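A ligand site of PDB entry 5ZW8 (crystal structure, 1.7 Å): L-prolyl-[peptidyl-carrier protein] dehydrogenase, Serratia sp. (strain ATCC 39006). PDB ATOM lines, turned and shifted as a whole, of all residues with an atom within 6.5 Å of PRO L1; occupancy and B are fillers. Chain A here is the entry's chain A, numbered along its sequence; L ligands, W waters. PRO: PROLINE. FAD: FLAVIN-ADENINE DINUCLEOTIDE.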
ATOM      1  N   THR A 128       7.655  -9.161   4.331  1.00  0.00           N
ATOM      2  CA  THR A 128       8.155  -8.453   5.523  1.00  0.00           C
ATOM      3  C   THR A 128       7.069  -7.825   6.360  1.00  0.00           C
ATOM      4  O   THR A 128       6.095  -7.285   5.819  1.00  0.00           O
ATOM      5  CB  THR A 128       9.138  -7.368   5.042  1.00  0.00           C
ATOM      6  OG1 THR A 128      10.165  -8.016   4.298  1.00  0.00           O
ATOM      7  CG2 THR A 128       9.726  -6.573   6.235  1.00  0.00           C
ATOM      8  N   GLY A 133      11.663  -9.167   9.854  1.00  0.00           N
ATOM      9  CA  GLY A 133      12.477  -8.715   8.720  1.00  0.00           C
ATOM     10  C   GLY A 133      13.480  -9.803   8.393  1.00  0.00           C
ATOM     11  O   GLY A 133      13.194 -10.768   7.679  1.00  0.00           O
ATOM     12  N   SER A 134      14.683  -9.720   9.012  1.00  0.00           N
ATOM     13  CA  SER A 134      15.606 -10.830   8.876  1.00  0.00           C
ATOM     14  C   SER A 134      14.997 -12.130   9.416  1.00  0.00           C
ATOM     15  O   SER A 134      15.262 -13.213   8.864  1.00  0.00           O
ATOM     16  CB  SER A 134      16.947 -10.547   9.590  1.00  0.00           C
ATOM     17  OG  SER A 134      17.495  -9.317   9.042  1.00  0.00           O
ATOM     18  N   ASP A 135      14.239 -12.034  10.494  1.00  0.00           N
ATOM     19  CA  ASP A 135      13.559 -13.187  11.102  1.00  0.00           C
ATOM     20  C   ASP A 135      12.203 -13.367  10.387  1.00  0.00           C
ATOM     21  O   ASP A 135      11.133 -13.296  11.013  1.00  0.00           O
ATOM     22  CB  ASP A 135      13.416 -12.928  12.598  1.00  0.00           C
ATOM     23  CG  ASP A 135      12.789 -14.107  13.409  1.00  0.00           C
ATOM     24  OD1 ASP A 135      12.705 -15.253  12.921  1.00  0.00           O
ATOM     25  OD2 ASP A 135      12.418 -13.793  14.563  1.00  0.00           O
ATOM     26  N   ILE A 136      12.284 -13.631   9.065  1.00  0.00           N
ATOM     27  CA  ILE A 136      11.079 -13.456   8.243  1.00  0.00           C
ATOM     28  C   ILE A 136      10.055 -14.547   8.570  1.00  0.00           C
ATOM     29  O   ILE A 136       8.834 -14.327   8.453  1.00  0.00           O
ATOM     30  CB  ILE A 136      11.484 -13.495   6.747  1.00  0.00           C
ATOM     31  CG1 ILE A 136      10.349 -13.068   5.841  1.00  0.00           C
ATOM     32  CG2 ILE A 136      11.923 -14.856   6.298  1.00  0.00           C
ATOM     33  CD1 ILE A 136       9.937 -11.679   6.120  1.00  0.00           C
ATOM     34  N   TYR A 137      10.524 -15.716   9.035  1.00  0.00           N
ATOM     35  CA  TYR A 137       9.600 -16.836   9.195  1.00  0.00           C
ATOM     36  C   TYR A 137       8.900 -16.747  10.536  1.00  0.00           C
ATOM     37  O   TYR A 137       8.001 -17.568  10.804  1.00  0.00           O
ATOM     38  CB  TYR A 137      10.302 -18.181   8.983  1.00  0.00           C
ATOM     39  CG  TYR A 137      10.978 -18.218   7.632  1.00  0.00           C
ATOM     40  CD1 TYR A 137      12.375 -18.140   7.526  1.00  0.00           C
ATOM     41  CD2 TYR A 137      10.221 -18.229   6.416  1.00  0.00           C
ATOM     42  CE1 TYR A 137      13.009 -18.098   6.277  1.00  0.00           C
ATOM     43  CE2 TYR A 137      10.867 -18.194   5.156  1.00  0.00           C
ATOM     44  CZ  TYR A 137      12.253 -18.108   5.099  1.00  0.00           C
ATOM     45  OH  TYR A 137      12.902 -18.065   3.884  1.00  0.00           O
ATOM     46  N   PHE A 180       8.988 -21.414   9.536  1.00  0.00           N
ATOM     47  CA  PHE A 180       9.198 -21.705   8.115  1.00  0.00           C
ATOM     48  C   PHE A 180       8.148 -22.669   7.547  1.00  0.00           C
ATOM     49  O   PHE A 180       7.588 -22.448   6.466  1.00  0.00           O
ATOM     50  CB  PHE A 180      10.604 -22.275   7.962  1.00  0.00           C
ATOM     51  CG  PHE A 180      10.991 -22.600   6.553  1.00  0.00           C
ATOM     52  CD1 PHE A 180      11.615 -21.623   5.734  1.00  0.00           C
ATOM     53  CD2 PHE A 180      10.816 -23.897   6.049  1.00  0.00           C
ATOM     54  CE1 PHE A 180      12.030 -21.938   4.414  1.00  0.00           C
ATOM     55  CE2 PHE A 180      11.187 -24.201   4.731  1.00  0.00           C
ATOM     56  CZ  PHE A 180      11.790 -23.218   3.912  1.00  0.00           C
ATOM     57  N   GLY A 234       7.173 -20.904   2.993  1.00  0.00           N
ATOM     58  CA  GLY A 234       8.536 -20.551   3.415  1.00  0.00           C
ATOM     59  C   GLY A 234       9.549 -20.911   2.345  1.00  0.00           C
ATOM     60  O   GLY A 234      10.433 -20.088   1.976  1.00  0.00           O
ATOM     61  N   PHE A 237       9.218 -18.665  -0.794  1.00  0.00           N
ATOM     62  CA  PHE A 237       9.809 -17.365  -0.568  1.00  0.00           C
ATOM     63  C   PHE A 237      11.316 -17.464  -0.663  1.00  0.00           C
ATOM     64  O   PHE A 237      11.981 -16.661  -1.329  1.00  0.00           O
ATOM     65  CB  PHE A 237       9.402 -16.812   0.781  1.00  0.00           C
ATOM     66  CG  PHE A 237      10.146 -15.556   1.176  1.00  0.00           C
ATOM     67  CD1 PHE A 237       9.755 -14.300   0.702  1.00  0.00           C
ATOM     68  CD2 PHE A 237      11.264 -15.640   1.997  1.00  0.00           C
ATOM     69  CE1 PHE A 237      10.449 -13.143   1.070  1.00  0.00           C
ATOM     70  CE2 PHE A 237      11.960 -14.477   2.373  1.00  0.00           C
ATOM     71  CZ  PHE A 237      11.545 -13.243   1.922  1.00  0.00           C
ATOM     72  N   HIS A 238      11.860 -18.453   0.005  1.00  0.00           N
ATOM     73  CA  HIS A 238      13.307 -18.630  -0.002  1.00  0.00           C
ATOM     74  C   HIS A 238      13.829 -18.827  -1.425  1.00  0.00           C
ATOM     75  O   HIS A 238      14.845 -18.219  -1.848  1.00  0.00           O
ATOM     76  CB  HIS A 238      13.642 -19.818   0.896  1.00  0.00           C
ATOM     77  CG  HIS A 238      15.122 -20.027   1.102  1.00  0.00           C
ATOM     78  ND1 HIS A 238      15.858 -19.261   1.986  1.00  0.00           N
ATOM     79  CD2 HIS A 238      15.986 -20.884   0.507  1.00  0.00           C
ATOM     80  CE1 HIS A 238      17.121 -19.660   1.938  1.00  0.00           C
ATOM     81  NE2 HIS A 238      17.230 -20.642   1.044  1.00  0.00           N
ATOM     82  N   MET A 241      13.942 -15.617  -3.304  1.00  0.00           N
ATOM     83  CA  MET A 241      15.069 -14.774  -2.878  1.00  0.00           C
ATOM     84  C   MET A 241      16.384 -15.213  -3.501  1.00  0.00           C
ATOM     85  O   MET A 241      17.266 -14.373  -3.716  1.00  0.00           O
ATOM     86  CB  MET A 241      15.193 -14.731  -1.350  1.00  0.00           C
ATOM     87  CG  MET A 241      13.992 -13.944  -0.703  1.00  0.00           C
ATOM     88  SD  MET A 241      13.840 -12.192  -1.246  1.00  0.00           S
ATOM     89  CE  MET A 241      12.312 -12.229  -2.280  1.00  0.00           C
ATOM     90  N   ILE A 242      16.527 -16.496  -3.817  1.00  0.00           N
ATOM     91  CA  ILE A 242      17.727 -16.836  -4.570  1.00  0.00           C
ATOM     92  C   ILE A 242      17.697 -16.197  -5.945  1.00  0.00           C
ATOM     93  O   ILE A 242      18.712 -15.647  -6.374  1.00  0.00           O
ATOM     94  CB  ILE A 242      17.908 -18.337  -4.709  1.00  0.00           C
ATOM     95  CG1 ILE A 242      17.764 -18.990  -3.336  1.00  0.00           C
ATOM     96  CG2 ILE A 242      19.311 -18.599  -5.401  1.00  0.00           C
ATOM     97  CD1 ILE A 242      17.819 -20.482  -3.389  1.00  0.00           C
ATOM     98  N   LYS A 245      18.358 -12.385  -5.345  1.00  0.00           N
ATOM     99  CA  LYS A 245      19.740 -12.020  -5.066  1.00  0.00           C
ATOM    100  C   LYS A 245      20.540 -11.979  -6.352  1.00  0.00           C
ATOM    101  O   LYS A 245      21.315 -11.035  -6.559  1.00  0.00           O
ATOM    102  CB  LYS A 245      20.343 -12.971  -4.041  1.00  0.00           C
ATOM    103  CG  LYS A 245      19.799 -12.608  -2.653  1.00  0.00           C
ATOM    104  CD  LYS A 245      20.495 -13.387  -1.538  1.00  0.00           C
ATOM    105  CE  LYS A 245      19.857 -14.771  -1.390  1.00  0.00           C
ATOM    106  NZ  LYS A 245      20.043 -15.324  -0.028  1.00  0.00           N
ATOM    107  N   GLU A 315      23.261 -22.255  -4.270  1.00  0.00           N
ATOM    108  CA  GLU A 315      22.733 -21.307  -3.307  1.00  0.00           C
ATOM    109  C   GLU A 315      23.845 -20.579  -2.555  1.00  0.00           C
ATOM    110  O   GLU A 315      23.758 -19.358  -2.346  1.00  0.00           O
ATOM    111  CB  GLU A 315      21.807 -22.002  -2.319  1.00  0.00           C
ATOM    112  CG  GLU A 315      21.284 -21.022  -1.266  1.00  0.00           C
ATOM    113  CD  GLU A 315      20.280 -21.656  -0.334  1.00  0.00           C
ATOM    114  OE1 GLU A 315      20.041 -22.889  -0.511  1.00  0.00           O
ATOM    115  OE2 GLU A 315      19.750 -20.942   0.556  1.00  0.00           O
ATOM    116  N   SER A 365      16.641  -8.441  -0.113  1.00  0.00           N
ATOM    117  CA  SER A 365      16.703  -9.878  -0.366  1.00  0.00           C
ATOM    118  C   SER A 365      17.446 -10.617   0.732  1.00  0.00           C
ATOM    119  O   SER A 365      17.960 -11.726   0.519  1.00  0.00           O
ATOM    120  CB  SER A 365      17.362 -10.210  -1.727  1.00  0.00           C
ATOM    121  OG  SER A 365      16.814  -9.434  -2.795  1.00  0.00           O
ATOM    122  N   GLY A 366      17.473 -10.039   1.913  1.00  0.00           N
ATOM    123  CA  GLY A 366      18.264 -10.628   2.999  1.00  0.00           C
ATOM    124  C   GLY A 366      19.494  -9.760   3.175  1.00  0.00           C
ATOM    125  O   GLY A 366      20.293  -9.607   2.241  1.00  0.00           O
ATOM    126  N   THR A 367      19.683  -9.198   4.370  1.00  0.00           N
ATOM    127  CA  THR A 367      20.839  -8.313   4.537  1.00  0.00           C
ATOM    128  C   THR A 367      22.148  -9.074   4.375  1.00  0.00           C
ATOM    129  O   THR A 367      22.214 -10.291   4.426  1.00  0.00           O
ATOM    130  CB  THR A 367      20.888  -7.703   5.946  1.00  0.00           C
ATOM    131  OG1 THR A 367      21.323  -8.705   6.868  1.00  0.00           O
ATOM    132  CG2 THR A 367      19.525  -7.084   6.452  1.00  0.00           C
ATOM    133  N   ILE A 370      22.793 -11.468   7.069  1.00  0.00           N
ATOM    134  CA  ILE A 370      22.077 -12.718   6.831  1.00  0.00           C
ATOM    135  C   ILE A 370      22.768 -13.543   5.722  1.00  0.00           C
ATOM    136  O   ILE A 370      22.800 -14.765   5.785  1.00  0.00           O
ATOM    137  CB  ILE A 370      20.601 -12.380   6.511  1.00  0.00           C
ATOM    138  CG1 ILE A 370      19.843 -11.924   7.784  1.00  0.00           C
ATOM    139  CG2 ILE A 370      19.886 -13.507   5.699  1.00  0.00           C
ATOM    140  CD1 ILE A 370      19.948 -12.909   8.885  1.00  0.00           C
ATOM    141  N   GLN A 371      23.311 -12.893   4.674  1.00  0.00           N
ATOM    142  CA  GLN A 371      24.037 -13.702   3.686  1.00  0.00           C
ATOM    143  C   GLN A 371      25.184 -14.438   4.356  1.00  0.00           C
ATOM    144  O   GLN A 371      25.494 -15.589   3.977  1.00  0.00           O
ATOM    145  CB  GLN A 371      24.615 -12.860   2.531  1.00  0.00           C
ATOM    146  CG  GLN A 371      23.507 -12.040   1.775  1.00  0.00           C
ATOM    147  CD  GLN A 371      22.316 -12.973   1.421  1.00  0.00           C
ATOM    148  OE1 GLN A 371      22.510 -14.084   0.908  1.00  0.00           O
ATOM    149  NE2 GLN A 371      21.114 -12.577   1.808  1.00  0.00           N
ATOM    150  N   ILE A 374      23.877 -17.443   6.007  1.00  0.00           N
ATOM    151  CA  ILE A 374      23.615 -18.489   5.015  1.00  0.00           C
ATOM    152  C   ILE A 374      24.917 -19.173   4.626  1.00  0.00           C
ATOM    153  O   ILE A 374      24.993 -20.398   4.591  1.00  0.00           O
ATOM    154  CB  ILE A 374      22.890 -17.869   3.800  1.00  0.00           C
ATOM    155  CG1 ILE A 374      21.519 -17.402   4.272  1.00  0.00           C
ATOM    156  CG2 ILE A 374      22.865 -18.899   2.600  1.00  0.00           C
ATOM    157  CD1 ILE A 374      20.725 -16.624   3.141  1.00  0.00           C
HETATM  158  N   PRO L   1      15.464 -14.364   5.085  1.00  0.00           N
HETATM  159  CA  PRO L   1      15.175 -14.658   3.662  1.00  0.00           C
HETATM  160  C   PRO L   1      15.868 -15.916   3.022  1.00  0.00           C
HETATM  161  O   PRO L   1      15.527 -17.020   3.490  1.00  0.00           O
HETATM  162  CB  PRO L   1      15.512 -13.325   2.977  1.00  0.00           C
HETATM  163  CG  PRO L   1      14.966 -12.206   4.055  1.00  0.00           C
HETATM  164  CD  PRO L   1      14.994 -12.994   5.457  1.00  0.00           C
HETATM  165  OXT PRO L   1      16.603 -15.985   2.032  1.00  0.00           O
HETATM  166  PA  FAD L   2      16.350  -6.152  10.649  1.00  0.00           P
HETATM  167  O1A FAD L   2      15.721  -5.411  11.810  1.00  0.00           O
HETATM  168  O2A FAD L   2      16.141  -7.566  10.413  1.00  0.00           O
HETATM  169  O5B FAD L   2      18.016  -5.940  10.674  1.00  0.00           O
HETATM  170  C5B FAD L   2      18.557  -4.888  11.495  1.00  0.00           C
HETATM  171  C4B FAD L   2      20.090  -5.295  11.650  1.00  0.00           C
HETATM  172  O4B FAD L   2      20.164  -6.458  12.354  1.00  0.00           O
HETATM  173  C3B FAD L   2      20.750  -5.518  10.293  1.00  0.00           C
HETATM  174  O3B FAD L   2      22.147  -5.115  10.346  1.00  0.00           O
HETATM  175  C2B FAD L   2      20.661  -7.069  10.241  1.00  0.00           C
HETATM  176  O2B FAD L   2      21.676  -7.591   9.311  1.00  0.00           O
HETATM  177  C1B FAD L   2      20.991  -7.409  11.558  1.00  0.00           C
HETATM  178  N9A FAD L   2      20.559  -8.748  11.947  1.00  0.00           N
HETATM  179  C8A FAD L   2      19.252  -9.259  12.075  1.00  0.00           C
HETATM  180  N7A FAD L   2      19.332 -10.560  12.319  1.00  0.00           N
HETATM  181  C5A FAD L   2      20.677 -10.850  12.411  1.00  0.00           C
HETATM  182  C6A FAD L   2      21.287 -12.033  12.661  1.00  0.00           C
HETATM  183  N6A FAD L   2      20.736 -13.325  12.937  1.00  0.00           N
HETATM  184  N1A FAD L   2      22.641 -12.107  12.659  1.00  0.00           N
HETATM  185  C2A FAD L   2      23.362 -10.980  12.398  1.00  0.00           C
HETATM  186  N3A FAD L   2      22.750  -9.825  12.171  1.00  0.00           N
HETATM  187  C4A FAD L   2      21.413  -9.757  12.186  1.00  0.00           C
HETATM  188  N1  FAD L   2      10.115  -6.880   1.852  1.00  0.00           N
HETATM  189  C2  FAD L   2       8.998  -7.564   1.208  1.00  0.00           C
HETATM  190  O2  FAD L   2       8.358  -8.359   1.823  1.00  0.00           O
HETATM  191  N3  FAD L   2       8.669  -7.199  -0.206  1.00  0.00           N
HETATM  192  C4  FAD L   2       9.368  -6.208  -0.951  1.00  0.00           C
HETATM  193  O4  FAD L   2       9.056  -5.837  -2.064  1.00  0.00           O
HETATM  194  C4X FAD L   2      10.539  -5.590  -0.228  1.00  0.00           C
HETATM  195  N5  FAD L   2      11.241  -4.642  -0.926  1.00  0.00           N
HETATM  196  C5X FAD L   2      12.360  -3.948  -0.304  1.00  0.00           C
HETATM  197  C6  FAD L   2      13.069  -2.990  -1.036  1.00  0.00           C
HETATM  198  C7  FAD L   2      14.129  -2.351  -0.357  1.00  0.00           C
HETATM  199  C7M FAD L   2      14.902  -1.316  -1.191  1.00  0.00           C
HETATM  200  C8  FAD L   2      14.447  -2.749   0.945  1.00  0.00           C
HETATM  201  C8M FAD L   2      15.701  -2.044   1.683  1.00  0.00           C
HETATM  202  C9  FAD L   2      13.776  -3.685   1.651  1.00  0.00           C
HETATM  203  C9A FAD L   2      12.704  -4.322   1.012  1.00  0.00           C
HETATM  204  N10 FAD L   2      11.965  -5.342   1.775  1.00  0.00           N
HETATM  205  C10 FAD L   2      10.877  -5.968   1.130  1.00  0.00           C
HETATM  206  C1' FAD L   2      12.309  -5.580   3.189  1.00  0.00           C
HETATM  207  C2' FAD L   2      13.540  -6.455   3.393  1.00  0.00           C
HETATM  208  O2' FAD L   2      13.085  -7.757   3.254  1.00  0.00           O
HETATM  209  C3' FAD L   2      13.998  -6.211   4.855  1.00  0.00           C
HETATM  210  O3' FAD L   2      14.328  -4.841   4.982  1.00  0.00           O
HETATM  211  C4' FAD L   2      15.208  -7.062   5.096  1.00  0.00           C
HETATM  212  O4' FAD L   2      14.870  -8.425   5.159  1.00  0.00           O
HETATM  213  C5' FAD L   2      15.815  -6.665   6.443  1.00  0.00           C
HETATM  214  O5' FAD L   2      14.793  -6.674   7.547  1.00  0.00           O
HETATM  215  P   FAD L   2      14.594  -5.421   8.454  1.00  0.00           P
HETATM  216  O1P FAD L   2      14.610  -4.157   7.663  1.00  0.00           O
HETATM  217  O2P FAD L   2      13.466  -5.615   9.405  1.00  0.00           O
HETATM  218  O3P FAD L   2      16.092  -5.341   9.255  1.00  0.00           O
HETATM  219  O   HOH W   1      18.570 -14.078   1.599  1.00  0.00           O
HETATM  220  O   HOH W   2      17.260 -17.278  -0.265  1.00  0.00           O
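The side-chain hydroxyl (OH) of Tyr 137 lies within hydrogen-bond range of an oxygen (O) of PRO L1 (2.9 Å).
An oxygen (O2) of FAD L2 is in hydrogen-bond range of the backbone NH (N) of Thr 128 (2.7 Å).
A ring nitrogen (ND1) of His 238 sits at hydrogen-bond distance from an oxygen (O) of PRO L1 (2.7 Å).
The side-chain hydroxyl of Thr 367 sits at hydrogen-bond distance from an oxygen (O2B) of FAD L2, 2.7 Å away.
N of Ser 134 is in hydrogen-bond range of O2A of FAD L2, 3.0 Å away.
OG of Ser 134 sits at hydrogen-bond distance from O2A of FAD L2 (2.6 Å).
The side-chain hydroxyl of Thr 128 lies within hydrogen-bond range of a nitrogen (N1) of FAD L2, at 2.7 Å.
The side-chain carboxylate (OE2) of Glu 315 is in hydrogen-bond range of a ring nitrogen (NE2) of His 238 (2.6 Å).
The side-chain amide nitrogen of Gln 371 is in hydrogen-bond range of the backbone carbonyl oxygen of Gly 366, at 3.1 Å.
Gly 133 touches PRO L1.
O of Ser 134 touches CD of PRO L1, at 3.4 Å.
Ile 136 touches PRO L1 (CG2 to CD, 3.7 Å).
Phe 237 touches PRO L1.
Met 241 touches PRO L1.
Ser 365 touches PRO L1.
Gly 366 touches PRO L1 (CA to CG, 3.8 Å).
Hydrophobic or aromatic side chains within 4 Å of PRO L1: Ile 136, Tyr 137, Phe 237, His 238 and Met 241.
Nine residues have an atom within 4 Å of PRO L1: Gly 133, Ser 134, Ile 136, Tyr 137, Phe 237, His 238, Met 241, Ser 365 and Gly 366.
The nearest printed residue that does not touch PRO L1 is Lys 245 (4.1 Å).
Water W2 lies within hydrogen-bond range of OXT of PRO L1, O of His 238 and NZ of Lys 245.
Water W1 lies within hydrogen-bond range of NZ of Lys 245 (2.5 Å), O of Ser 365 (2.7 Å), OXT of PRO L1 (2.8 Å) and NE2 of Gln 371 (3.0 Å).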
